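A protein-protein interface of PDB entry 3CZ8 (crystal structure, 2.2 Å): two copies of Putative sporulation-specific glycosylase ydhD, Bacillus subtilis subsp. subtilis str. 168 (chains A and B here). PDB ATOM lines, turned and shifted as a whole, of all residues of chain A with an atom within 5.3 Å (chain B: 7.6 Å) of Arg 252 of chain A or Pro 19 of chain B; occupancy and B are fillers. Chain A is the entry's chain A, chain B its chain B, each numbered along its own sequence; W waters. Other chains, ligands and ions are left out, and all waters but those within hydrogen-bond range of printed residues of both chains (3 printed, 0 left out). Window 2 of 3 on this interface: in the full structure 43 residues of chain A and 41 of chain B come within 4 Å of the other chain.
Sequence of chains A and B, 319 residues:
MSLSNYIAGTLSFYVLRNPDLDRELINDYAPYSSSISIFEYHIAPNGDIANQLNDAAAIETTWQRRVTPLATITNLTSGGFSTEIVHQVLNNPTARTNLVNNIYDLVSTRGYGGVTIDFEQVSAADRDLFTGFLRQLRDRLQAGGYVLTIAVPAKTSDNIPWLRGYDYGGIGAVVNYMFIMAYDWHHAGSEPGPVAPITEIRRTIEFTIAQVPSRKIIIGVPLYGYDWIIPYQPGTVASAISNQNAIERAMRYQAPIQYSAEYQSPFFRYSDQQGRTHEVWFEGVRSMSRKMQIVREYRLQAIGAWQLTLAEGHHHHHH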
ATOM      1  N   GLU A 248       0.785   7.474  -4.744  1.00  0.00           N
ATOM      2  CA  GLU A 248       1.585   6.527  -3.965  1.00  0.00           C
ATOM      3  C   GLU A 248       0.783   5.316  -3.482  1.00  0.00           C
ATOM      4  O   GLU A 248       1.311   4.204  -3.442  1.00  0.00           O
ATOM      5  CB  GLU A 248       2.248   7.234  -2.780  1.00  0.00           C
ATOM      6  CG  GLU A 248       3.430   8.133  -3.188  1.00  0.00           C
ATOM      7  CD  GLU A 248       3.769   9.198  -2.149  1.00  0.00           C
ATOM      8  OE1 GLU A 248       3.048   9.328  -1.129  1.00  0.00           O
ATOM      9  OE2 GLU A 248       4.768   9.913  -2.358  1.00  0.00           O
ATOM     10  N   ARG A 249      -0.484   5.531  -3.130  1.00  0.00           N
ATOM     11  CA  ARG A 249      -1.376   4.436  -2.727  1.00  0.00           C
ATOM     12  C   ARG A 249      -1.829   3.589  -3.908  1.00  0.00           C
ATOM     13  O   ARG A 249      -2.012   2.384  -3.769  1.00  0.00           O
ATOM     14  CB  ARG A 249      -2.581   4.961  -1.954  1.00  0.00           C
ATOM     15  CG  ARG A 249      -2.218   5.449  -0.570  1.00  0.00           C
ATOM     16  CD  ARG A 249      -3.435   5.824   0.244  1.00  0.00           C
ATOM     17  NE  ARG A 249      -3.036   6.391   1.530  1.00  0.00           N
ATOM     18  CZ  ARG A 249      -3.801   6.425   2.616  1.00  0.00           C
ATOM     19  NH1 ARG A 249      -5.027   5.921   2.594  1.00  0.00           N
ATOM     20  NH2 ARG A 249      -3.331   6.965   3.732  1.00  0.00           N
ATOM     21  N   ALA A 250      -2.003   4.217  -5.068  1.00  0.00           N
ATOM     22  CA  ALA A 250      -2.331   3.498  -6.299  1.00  0.00           C
ATOM     23  C   ALA A 250      -1.207   2.555  -6.737  1.00  0.00           C
ATOM     24  O   ALA A 250      -1.479   1.520  -7.326  1.00  0.00           O
ATOM     25  CB  ALA A 250      -2.685   4.474  -7.420  1.00  0.00           C
ATOM     26  N   MET A 251       0.043   2.919  -6.441  1.00  0.00           N
ATOM     27  CA  MET A 251       1.211   2.077  -6.747  1.00  0.00           C
ATOM     28  C   MET A 251       1.293   0.863  -5.834  1.00  0.00           C
ATOM     29  O   MET A 251       1.430  -0.264  -6.313  1.00  0.00           O
ATOM     30  CB  MET A 251       2.515   2.857  -6.592  1.00  0.00           C
ATOM     31  CG  MET A 251       2.688   4.038  -7.504  1.00  0.00           C
ATOM     32  SD  MET A 251       4.399   4.581  -7.570  1.00  0.00           S
ATOM     33  CE  MET A 251       4.993   4.394  -5.880  1.00  0.00           C
ATOM     34  N   ARG A 252       1.228   1.116  -4.524  1.00  0.00           N
ATOM     35  CA  ARG A 252       1.284   0.084  -3.482  1.00  0.00           C
ATOM     36  C   ARG A 252       0.230  -1.015  -3.676  1.00  0.00           C
ATOM     37  O   ARG A 252       0.511  -2.198  -3.458  1.00  0.00           O
ATOM     38  CB  ARG A 252       1.155   0.729  -2.090  1.00  0.00           C
ATOM     39  CG  ARG A 252       1.445  -0.190  -0.891  1.00  0.00           C
ATOM     40  CD  ARG A 252       0.160  -0.688  -0.250  1.00  0.00           C
ATOM     41  NE  ARG A 252       0.343  -1.778   0.708  1.00  0.00           N
ATOM     42  CZ  ARG A 252       0.322  -3.074   0.397  1.00  0.00           C
ATOM     43  NH1 ARG A 252       0.147  -3.472  -0.862  1.00  0.00           N
ATOM     44  NH2 ARG A 252       0.487  -3.980   1.351  1.00  0.00           N
ATOM     45  N   TYR A 253      -0.972  -0.618  -4.090  1.00  0.00           N
ATOM     46  CA  TYR A 253      -2.071  -1.562  -4.268  1.00  0.00           C
ATOM     47  C   TYR A 253      -2.256  -1.988  -5.721  1.00  0.00           C
ATOM     48  O   TYR A 253      -3.126  -2.812  -6.022  1.00  0.00           O
ATOM     49  CB  TYR A 253      -3.370  -0.988  -3.696  1.00  0.00           C
ATOM     50  CG  TYR A 253      -3.352  -0.839  -2.188  1.00  0.00           C
ATOM     51  CD1 TYR A 253      -3.508  -1.951  -1.352  1.00  0.00           C
ATOM     52  CD2 TYR A 253      -3.182   0.412  -1.595  1.00  0.00           C
ATOM     53  CE1 TYR A 253      -3.489  -1.814   0.039  1.00  0.00           C
ATOM     54  CE2 TYR A 253      -3.160   0.559  -0.207  1.00  0.00           C
ATOM     55  CZ  TYR A 253      -3.318  -0.560   0.602  1.00  0.00           C
ATOM     56  OH  TYR A 253      -3.300  -0.422   1.970  1.00  0.00           O
ATOM     57  N   GLN A 254      -1.425  -1.426  -6.602  1.00  0.00           N
ATOM     58  CA  GLN A 254      -1.448  -1.679  -8.055  1.00  0.00           C
ATOM     59  C   GLN A 254      -2.823  -1.444  -8.686  1.00  0.00           C
ATOM     60  O   GLN A 254      -3.260  -2.188  -9.572  1.00  0.00           O
ATOM     61  CB  GLN A 254      -0.866  -3.062  -8.405  1.00  0.00           C
ATOM     62  CG  GLN A 254       0.652  -3.160  -8.212  1.00  0.00           C
ATOM     63  CD  GLN A 254       1.431  -2.304  -9.201  1.00  0.00           C
ATOM     64  OE1 GLN A 254       1.339  -2.499 -10.412  1.00  0.00           O
ATOM     65  NE2 GLN A 254       2.209  -1.359  -8.686  1.00  0.00           N
ATOM     66  N   GLN A 273      -5.403  -4.930   2.983  1.00  0.00           N
ATOM     67  CA  GLN A 273      -4.954  -6.195   3.571  1.00  0.00           C
ATOM     68  C   GLN A 273      -5.937  -6.774   4.591  1.00  0.00           C
ATOM     69  O   GLN A 273      -5.589  -7.682   5.356  1.00  0.00           O
ATOM     70  CB  GLN A 273      -3.575  -6.010   4.219  1.00  0.00           C
ATOM     71  CG  GLN A 273      -2.401  -6.146   3.257  1.00  0.00           C
ATOM     72  CD  GLN A 273      -1.909  -7.578   3.130  1.00  0.00           C
ATOM     73  OE1 GLN A 273      -1.345  -8.139   4.070  1.00  0.00           O
ATOM     74  NE2 GLN A 273      -2.111  -8.171   1.959  1.00  0.00           N
ATOM     75  N   TYR B  14       6.373   7.527   5.696  1.00  0.00           N
ATOM     76  CA  TYR B  14       5.564   6.316   5.744  1.00  0.00           C
ATOM     77  C   TYR B  14       5.970   5.268   4.702  1.00  0.00           C
ATOM     78  O   TYR B  14       6.644   5.581   3.723  1.00  0.00           O
ATOM     79  CB  TYR B  14       4.071   6.655   5.703  1.00  0.00           C
ATOM     80  CG  TYR B  14       3.501   6.899   4.332  1.00  0.00           C
ATOM     81  CD1 TYR B  14       2.588   6.005   3.782  1.00  0.00           C
ATOM     82  CD2 TYR B  14       3.859   8.025   3.588  1.00  0.00           C
ATOM     83  CE1 TYR B  14       2.053   6.214   2.521  1.00  0.00           C
ATOM     84  CE2 TYR B  14       3.326   8.246   2.321  1.00  0.00           C
ATOM     85  CZ  TYR B  14       2.428   7.334   1.795  1.00  0.00           C
ATOM     86  OH  TYR B  14       1.889   7.528   0.544  1.00  0.00           O
ATOM     87  N   VAL B  15       5.542   4.029   4.929  1.00  0.00           N
ATOM     88  CA  VAL B  15       6.027   2.871   4.178  1.00  0.00           C
ATOM     89  C   VAL B  15       4.971   2.327   3.210  1.00  0.00           C
ATOM     90  O   VAL B  15       3.859   1.989   3.623  1.00  0.00           O
ATOM     91  CB  VAL B  15       6.542   1.763   5.167  1.00  0.00           C
ATOM     92  CG1 VAL B  15       6.776   0.424   4.473  1.00  0.00           C
ATOM     93  CG2 VAL B  15       7.815   2.228   5.865  1.00  0.00           C
ATOM     94  N   LEU B  16       5.331   2.271   1.923  1.00  0.00           N
ATOM     95  CA  LEU B  16       4.495   1.688   0.869  1.00  0.00           C
ATOM     96  C   LEU B  16       5.065   0.337   0.472  1.00  0.00           C
ATOM     97  O   LEU B  16       6.003   0.266  -0.336  1.00  0.00           O
ATOM     98  CB  LEU B  16       4.479   2.560  -0.392  1.00  0.00           C
ATOM     99  CG  LEU B  16       3.808   3.926  -0.568  1.00  0.00           C
ATOM    100  CD1 LEU B  16       2.332   3.909  -0.179  1.00  0.00           C
ATOM    101  CD2 LEU B  16       4.574   5.017   0.154  1.00  0.00           C
ATOM    102  N   ARG B  17       4.474  -0.722   1.015  1.00  0.00           N
ATOM    103  CA  ARG B  17       4.933  -2.096   0.809  1.00  0.00           C
ATOM    104  C   ARG B  17       4.981  -2.524  -0.656  1.00  0.00           C
ATOM    105  O   ARG B  17       4.087  -2.190  -1.438  1.00  0.00           O
ATOM    106  CB  ARG B  17       4.027  -3.051   1.581  1.00  0.00           C
ATOM    107  CG  ARG B  17       4.683  -4.349   1.998  1.00  0.00           C
ATOM    108  CD  ARG B  17       3.638  -5.297   2.535  1.00  0.00           C
ATOM    109  NE  ARG B  17       4.215  -6.396   3.300  1.00  0.00           N
ATOM    110  CZ  ARG B  17       3.517  -7.430   3.761  1.00  0.00           C
ATOM    111  NH1 ARG B  17       2.209  -7.513   3.530  1.00  0.00           N
ATOM    112  NH2 ARG B  17       4.129  -8.384   4.449  1.00  0.00           N
ATOM    113  N   ASN B  18       6.063  -3.221  -1.008  1.00  0.00           N
ATOM    114  CA  ASN B  18       6.176  -4.007  -2.239  1.00  0.00           C
ATOM    115  C   ASN B  18       4.962  -4.937  -2.314  1.00  0.00           C
ATOM    116  O   ASN B  18       4.800  -5.797  -1.446  1.00  0.00           O
ATOM    117  CB  ASN B  18       7.489  -4.807  -2.166  1.00  0.00           C
ATOM    118  CG  ASN B  18       7.787  -5.646  -3.399  1.00  0.00           C
ATOM    119  OD1 ASN B  18       6.941  -5.878  -4.259  1.00  0.00           O
ATOM    120  ND2 ASN B  18       9.024  -6.126  -3.470  1.00  0.00           N
ATOM    121  N   PRO B  19       4.093  -4.749  -3.334  1.00  0.00           N
ATOM    122  CA  PRO B  19       2.865  -5.552  -3.478  1.00  0.00           C
ATOM    123  C   PRO B  19       3.085  -7.053  -3.713  1.00  0.00           C
ATOM    124  O   PRO B  19       2.151  -7.837  -3.534  1.00  0.00           O
ATOM    125  CB  PRO B  19       2.157  -4.916  -4.684  1.00  0.00           C
ATOM    126  CG  PRO B  19       3.221  -4.205  -5.434  1.00  0.00           C
ATOM    127  CD  PRO B  19       4.216  -3.744  -4.407  1.00  0.00           C
ATOM    128  N   ASP B  20       4.302  -7.449  -4.092  1.00  0.00           N
ATOM    129  CA  ASP B  20       4.651  -8.864  -4.256  1.00  0.00           C
ATOM    130  C   ASP B  20       4.709  -9.608  -2.917  1.00  0.00           C
ATOM    131  O   ASP B  20       4.655 -10.839  -2.880  1.00  0.00           O
ATOM    132  CB  ASP B  20       5.985  -9.018  -5.003  1.00  0.00           C
ATOM    133  CG  ASP B  20       5.917  -8.530  -6.446  1.00  0.00           C
ATOM    134  OD1 ASP B  20       6.948  -8.051  -6.962  1.00  0.00           O
ATOM    135  OD2 ASP B  20       4.841  -8.622  -7.071  1.00  0.00           O
ATOM    136  N   LEU B  21       4.803  -8.851  -1.825  1.00  0.00           N
ATOM    137  CA  LEU B  21       4.889  -9.416  -0.479  1.00  0.00           C
ATOM    138  C   LEU B  21       3.517  -9.626   0.189  1.00  0.00           C
ATOM    139  O   LEU B  21       3.443  -9.976   1.371  1.00  0.00           O
ATOM    140  CB  LEU B  21       5.782  -8.537   0.414  1.00  0.00           C
ATOM    141  CG  LEU B  21       7.144  -8.020  -0.062  1.00  0.00           C
ATOM    142  CD1 LEU B  21       7.873  -7.349   1.099  1.00  0.00           C
ATOM    143  CD2 LEU B  21       8.013  -9.111  -0.675  1.00  0.00           C
ATOM    144  N   ASP B  22       2.443  -9.411  -0.565  1.00  0.00           N
ATOM    145  CA  ASP B  22       1.083  -9.555  -0.045  1.00  0.00           C
ATOM    146  C   ASP B  22       0.530 -10.968  -0.242  1.00  0.00           C
ATOM    147  O   ASP B  22       1.251 -11.957  -0.108  1.00  0.00           O
ATOM    148  CB  ASP B  22       0.146  -8.537  -0.705  1.00  0.00           C
ATOM    149  CG  ASP B  22       0.394  -7.108  -0.238  1.00  0.00           C
ATOM    150  OD1 ASP B  22       1.043  -6.898   0.814  1.00  0.00           O
ATOM    151  OD2 ASP B  22      -0.079  -6.186  -0.930  1.00  0.00           O
ATOM    152  N   SER B  33       1.850  -5.074   6.331  1.00  0.00           N
ATOM    153  CA  SER B  33       2.183  -4.215   7.466  1.00  0.00           C
ATOM    154  C   SER B  33       2.923  -2.950   7.019  1.00  0.00           C
ATOM    155  O   SER B  33       3.698  -2.977   6.058  1.00  0.00           O
ATOM    156  CB  SER B  33       3.009  -4.985   8.501  1.00  0.00           C
ATOM    157  OG  SER B  33       3.101  -4.265   9.720  1.00  0.00           O
ATOM    158  N   SER B  34       2.677  -1.848   7.726  1.00  0.00           N
ATOM    159  CA  SER B  34       3.244  -0.545   7.378  1.00  0.00           C
ATOM    160  C   SER B  34       3.607   0.256   8.625  1.00  0.00           C
ATOM    161  O   SER B  34       3.161  -0.057   9.732  1.00  0.00           O
ATOM    162  CB  SER B  34       2.260   0.245   6.506  1.00  0.00           C
ATOM    163  OG  SER B  34       2.761   1.531   6.177  1.00  0.00           O
ATOM    164  N   MET B 292       8.933   2.082  -7.851  1.00  0.00           N
ATOM    165  CA  MET B 292       8.293   0.867  -7.338  1.00  0.00           C
ATOM    166  C   MET B 292       8.679  -0.376  -8.156  1.00  0.00           C
ATOM    167  O   MET B 292       8.852  -1.453  -7.591  1.00  0.00           O
ATOM    168  CB  MET B 292       6.766   1.009  -7.216  1.00  0.00           C
ATOM    169  CG  MET B 292       6.061  -0.226  -6.590  1.00  0.00           C
ATOM    170  SD  MET B 292       6.690  -0.789  -4.978  1.00  0.00           S
ATOM    171  CE  MET B 292       5.661   0.186  -3.882  1.00  0.00           C
ATOM    172  N   VAL B 295      12.061  -1.572  -7.061  1.00  0.00           N
ATOM    173  CA  VAL B 295      11.881  -2.175  -5.737  1.00  0.00           C
ATOM    174  C   VAL B 295      11.436  -3.630  -5.914  1.00  0.00           C
ATOM    175  O   VAL B 295      11.994  -4.539  -5.300  1.00  0.00           O
ATOM    176  CB  VAL B 295      10.887  -1.345  -4.864  1.00  0.00           C
ATOM    177  CG1 VAL B 295      10.236  -2.187  -3.756  1.00  0.00           C
ATOM    178  CG2 VAL B 295      11.593  -0.141  -4.264  1.00  0.00           C
ATOM    179  N   ARG B 296      10.467  -3.832  -6.800  1.00  0.00           N
ATOM    180  CA  ARG B 296       9.922  -5.147  -7.093  1.00  0.00           C
ATOM    181  C   ARG B 296      10.900  -6.053  -7.854  1.00  0.00           C
ATOM    182  O   ARG B 296      10.870  -7.271  -7.677  1.00  0.00           O
ATOM    183  CB  ARG B 296       8.619  -5.006  -7.874  1.00  0.00           C
ATOM    184  CG  ARG B 296       7.503  -4.321  -7.104  1.00  0.00           C
ATOM    185  CD  ARG B 296       6.278  -4.149  -7.976  1.00  0.00           C
ATOM    186  NE  ARG B 296       5.495  -5.379  -8.057  1.00  0.00           N
ATOM    187  CZ  ARG B 296       4.526  -5.602  -8.941  1.00  0.00           C
ATOM    188  NH1 ARG B 296       4.209  -4.682  -9.841  1.00  0.00           N
ATOM    189  NH2 ARG B 296       3.867  -6.751  -8.925  1.00  0.00           N
ATOM    190  N   LEU B 300      12.866  -5.943  -2.926  1.00  0.00           N
ATOM    191  CA  LEU B 300      13.069  -5.150  -1.711  1.00  0.00           C
ATOM    192  C   LEU B 300      11.751  -5.004  -0.956  1.00  0.00           C
ATOM    193  O   LEU B 300      10.687  -5.377  -1.469  1.00  0.00           O
ATOM    194  CB  LEU B 300      13.673  -3.777  -2.044  1.00  0.00           C
ATOM    195  CG  LEU B 300      14.877  -3.726  -2.996  1.00  0.00           C
ATOM    196  CD1 LEU B 300      15.298  -2.286  -3.267  1.00  0.00           C
ATOM    197  CD2 LEU B 300      16.054  -4.534  -2.440  1.00  0.00           C
ATOM    198  N   GLN B 301      11.832  -4.464   0.260  1.00  0.00           N
ATOM    199  CA  GLN B 301      10.689  -4.420   1.176  1.00  0.00           C
ATOM    200  C   GLN B 301       9.591  -3.464   0.714  1.00  0.00           C
ATOM    201  O   GLN B 301       8.409  -3.822   0.723  1.00  0.00           O
ATOM    202  CB  GLN B 301      11.159  -4.041   2.592  1.00  0.00           C
ATOM    203  CG  GLN B 301      10.079  -4.009   3.680  1.00  0.00           C
ATOM    204  CD  GLN B 301       9.404  -5.357   3.916  1.00  0.00           C
ATOM    205  OE1 GLN B 301      10.062  -6.391   4.024  1.00  0.00           O
ATOM    206  NE2 GLN B 301       8.080  -5.342   4.004  1.00  0.00           N
ATOM    207  N   ALA B 302       9.993  -2.262   0.297  1.00  0.00           N
ATOM    208  CA  ALA B 302       9.059  -1.153   0.165  1.00  0.00           C
ATOM    209  C   ALA B 302       9.644   0.124  -0.433  1.00  0.00           C
ATOM    210  O   ALA B 302      10.868   0.299  -0.544  1.00  0.00           O
ATOM    211  CB  ALA B 302       8.460  -0.837   1.542  1.00  0.00           C
ATOM    212  N   ILE B 303       8.731   1.009  -0.819  1.00  0.00           N
ATOM    213  CA  ILE B 303       9.023   2.407  -1.099  1.00  0.00           C
ATOM    214  C   ILE B 303       8.701   3.193   0.188  1.00  0.00           C
ATOM    215  O   ILE B 303       7.713   2.907   0.866  1.00  0.00           O
ATOM    216  CB  ILE B 303       8.163   2.909  -2.300  1.00  0.00           C
ATOM    217  CG1 ILE B 303       8.782   2.472  -3.637  1.00  0.00           C
ATOM    218  CG2 ILE B 303       7.954   4.424  -2.271  1.00  0.00           C
ATOM    219  CD1 ILE B 303       9.998   3.273  -4.077  1.00  0.00           C
HETATM  220  O   HOH W   1      -0.039  -3.015   4.383  1.00  0.00           O
HETATM  221  O   HOH W   2       2.060  -0.249   2.958  1.00  0.00           O
HETATM  222  O   HOH W   3      -0.654   7.768   1.352  1.00  0.00           O
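The side-chain carboxylate (OE1) of Glu 248 of chain A lies within hydrogen-bond range of the side-chain hydroxyl (OH) of Tyr 14 of chain B, at 2.7 Å.
OD2 of Asp 22 of chain B lies within salt-bridge range of NH1 of Arg 252 of chain A (2.7 Å).
The backbone carbonyl oxygen of Met 251 of chain A is in hydrogen-bond range of the side-chain amide nitrogen of Gln 254 of chain A, at 2.7 Å.
O of Ile 303 of chain B lies within hydrogen-bond range of N of Leu 16 of chain B.
The guanidinium group (NH1) of Arg 17 of chain B lies close to the backbone carbonyl oxygen (O) of Leu 21 of chain B.
The guanidinium group of Arg 17 of chain B lies within salt-bridge range of the side-chain carboxylate of Asp 22 of chain B (3.0 Å).
The side-chain carboxylate of Asp 20 of chain B is in salt-bridge range of the guanidinium group of Arg 296 of chain B.
O of Glu 248 of chain A touches CD1 of Leu 16 of chain B, at 3.4 Å.
CB of Arg 252 of chain A touches CD1 of Leu 16 of chain B (3.9 Å).
Arg 17 of chain B touches Arg 252 of chain A (O to CG, 3.4 Å).
O of Arg 252 of chain A touches CB of Pro 19 of chain B, at 3.4 Å.
Gln 254 of chain A touches Pro 19 of chain B (CG to CG, 3.9 Å).
Arg 296 of chain B touches Gln 254 of chain A.
Gln 273 of chain A touches Arg 17 of chain B.
Asp 22 of chain B touches Gln 273 of chain A (CG to NE2, 3.5 Å).
Of chain B, only Leu 16 (3.9 Å), Arg 17 (3.4 Å), Pro 19 (3.4 Å) and Asp 22 (2.7 Å) come within 4 Å of Arg 252 of chain A.
Of chain A, only Arg 252 (3.4 Å) and Gln 254 (3.9 Å) come within 4 Å of Pro 19 of chain B.
Printed residues of chain A within 4 Å of Arg 17 of chain B: Arg 252 (3.4 Å) and Gln 273 (3.6 Å).
Of the printed residues of chain B, Gln 273 of chain A touches Arg 17 and Asp 22.
Of the printed residues of chain A, Tyr 14 of chain B touches Glu 248.
Of the printed residues of chain A, Arg 296 of chain B touches Gln 254.
Printed residues of chain A within 4 Å of Leu 16 of chain B: Glu 248 and Arg 252.
The nearest residue of chain A that does not touch Pro 19 of chain B is Met 251 of chain A (4.4 Å).
Hydrophobic or aromatic side chains of chain B within 4 Å of the printed part of chain A: Tyr 14, Leu 16 and Pro 19.
Along chain B the printed residues that touch a printed residue of chain A span positions 14 to 296.
Of the 8 printed residues of chain A, 4 touch a printed residue of chain B.
Along chain A the printed residues that touch a printed residue of chain B span positions 248 to 273.
Among the printed residues, 10 pairs touch across the chains.
Among the printed residues, Asp or Glu carboxylates within 4 Å of a Lys or Arg side-chain nitrogen of the other chain: Arg 252 of chain A with Asp 22 of chain B (2.7 Å).
No position is printed for both chains.
Water W3 bridges OH of Tyr 14 of chain B (2.7 Å) and NE of Arg 249 of chain A (2.8 Å).
Water W2 lies within hydrogen-bond range of the backbone carbonyl oxygen of Val 15 of chain B (2.9 Å), the backbone NH of Arg 17 of chain B (3.1 Å) and the guanidinium group of Arg 252 of chain A (3.2 Å).
Water W1 bridges NH2 of Arg 252 of chain A (3.2 Å) and N of Ser 33 of chain B (3.4 Å).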
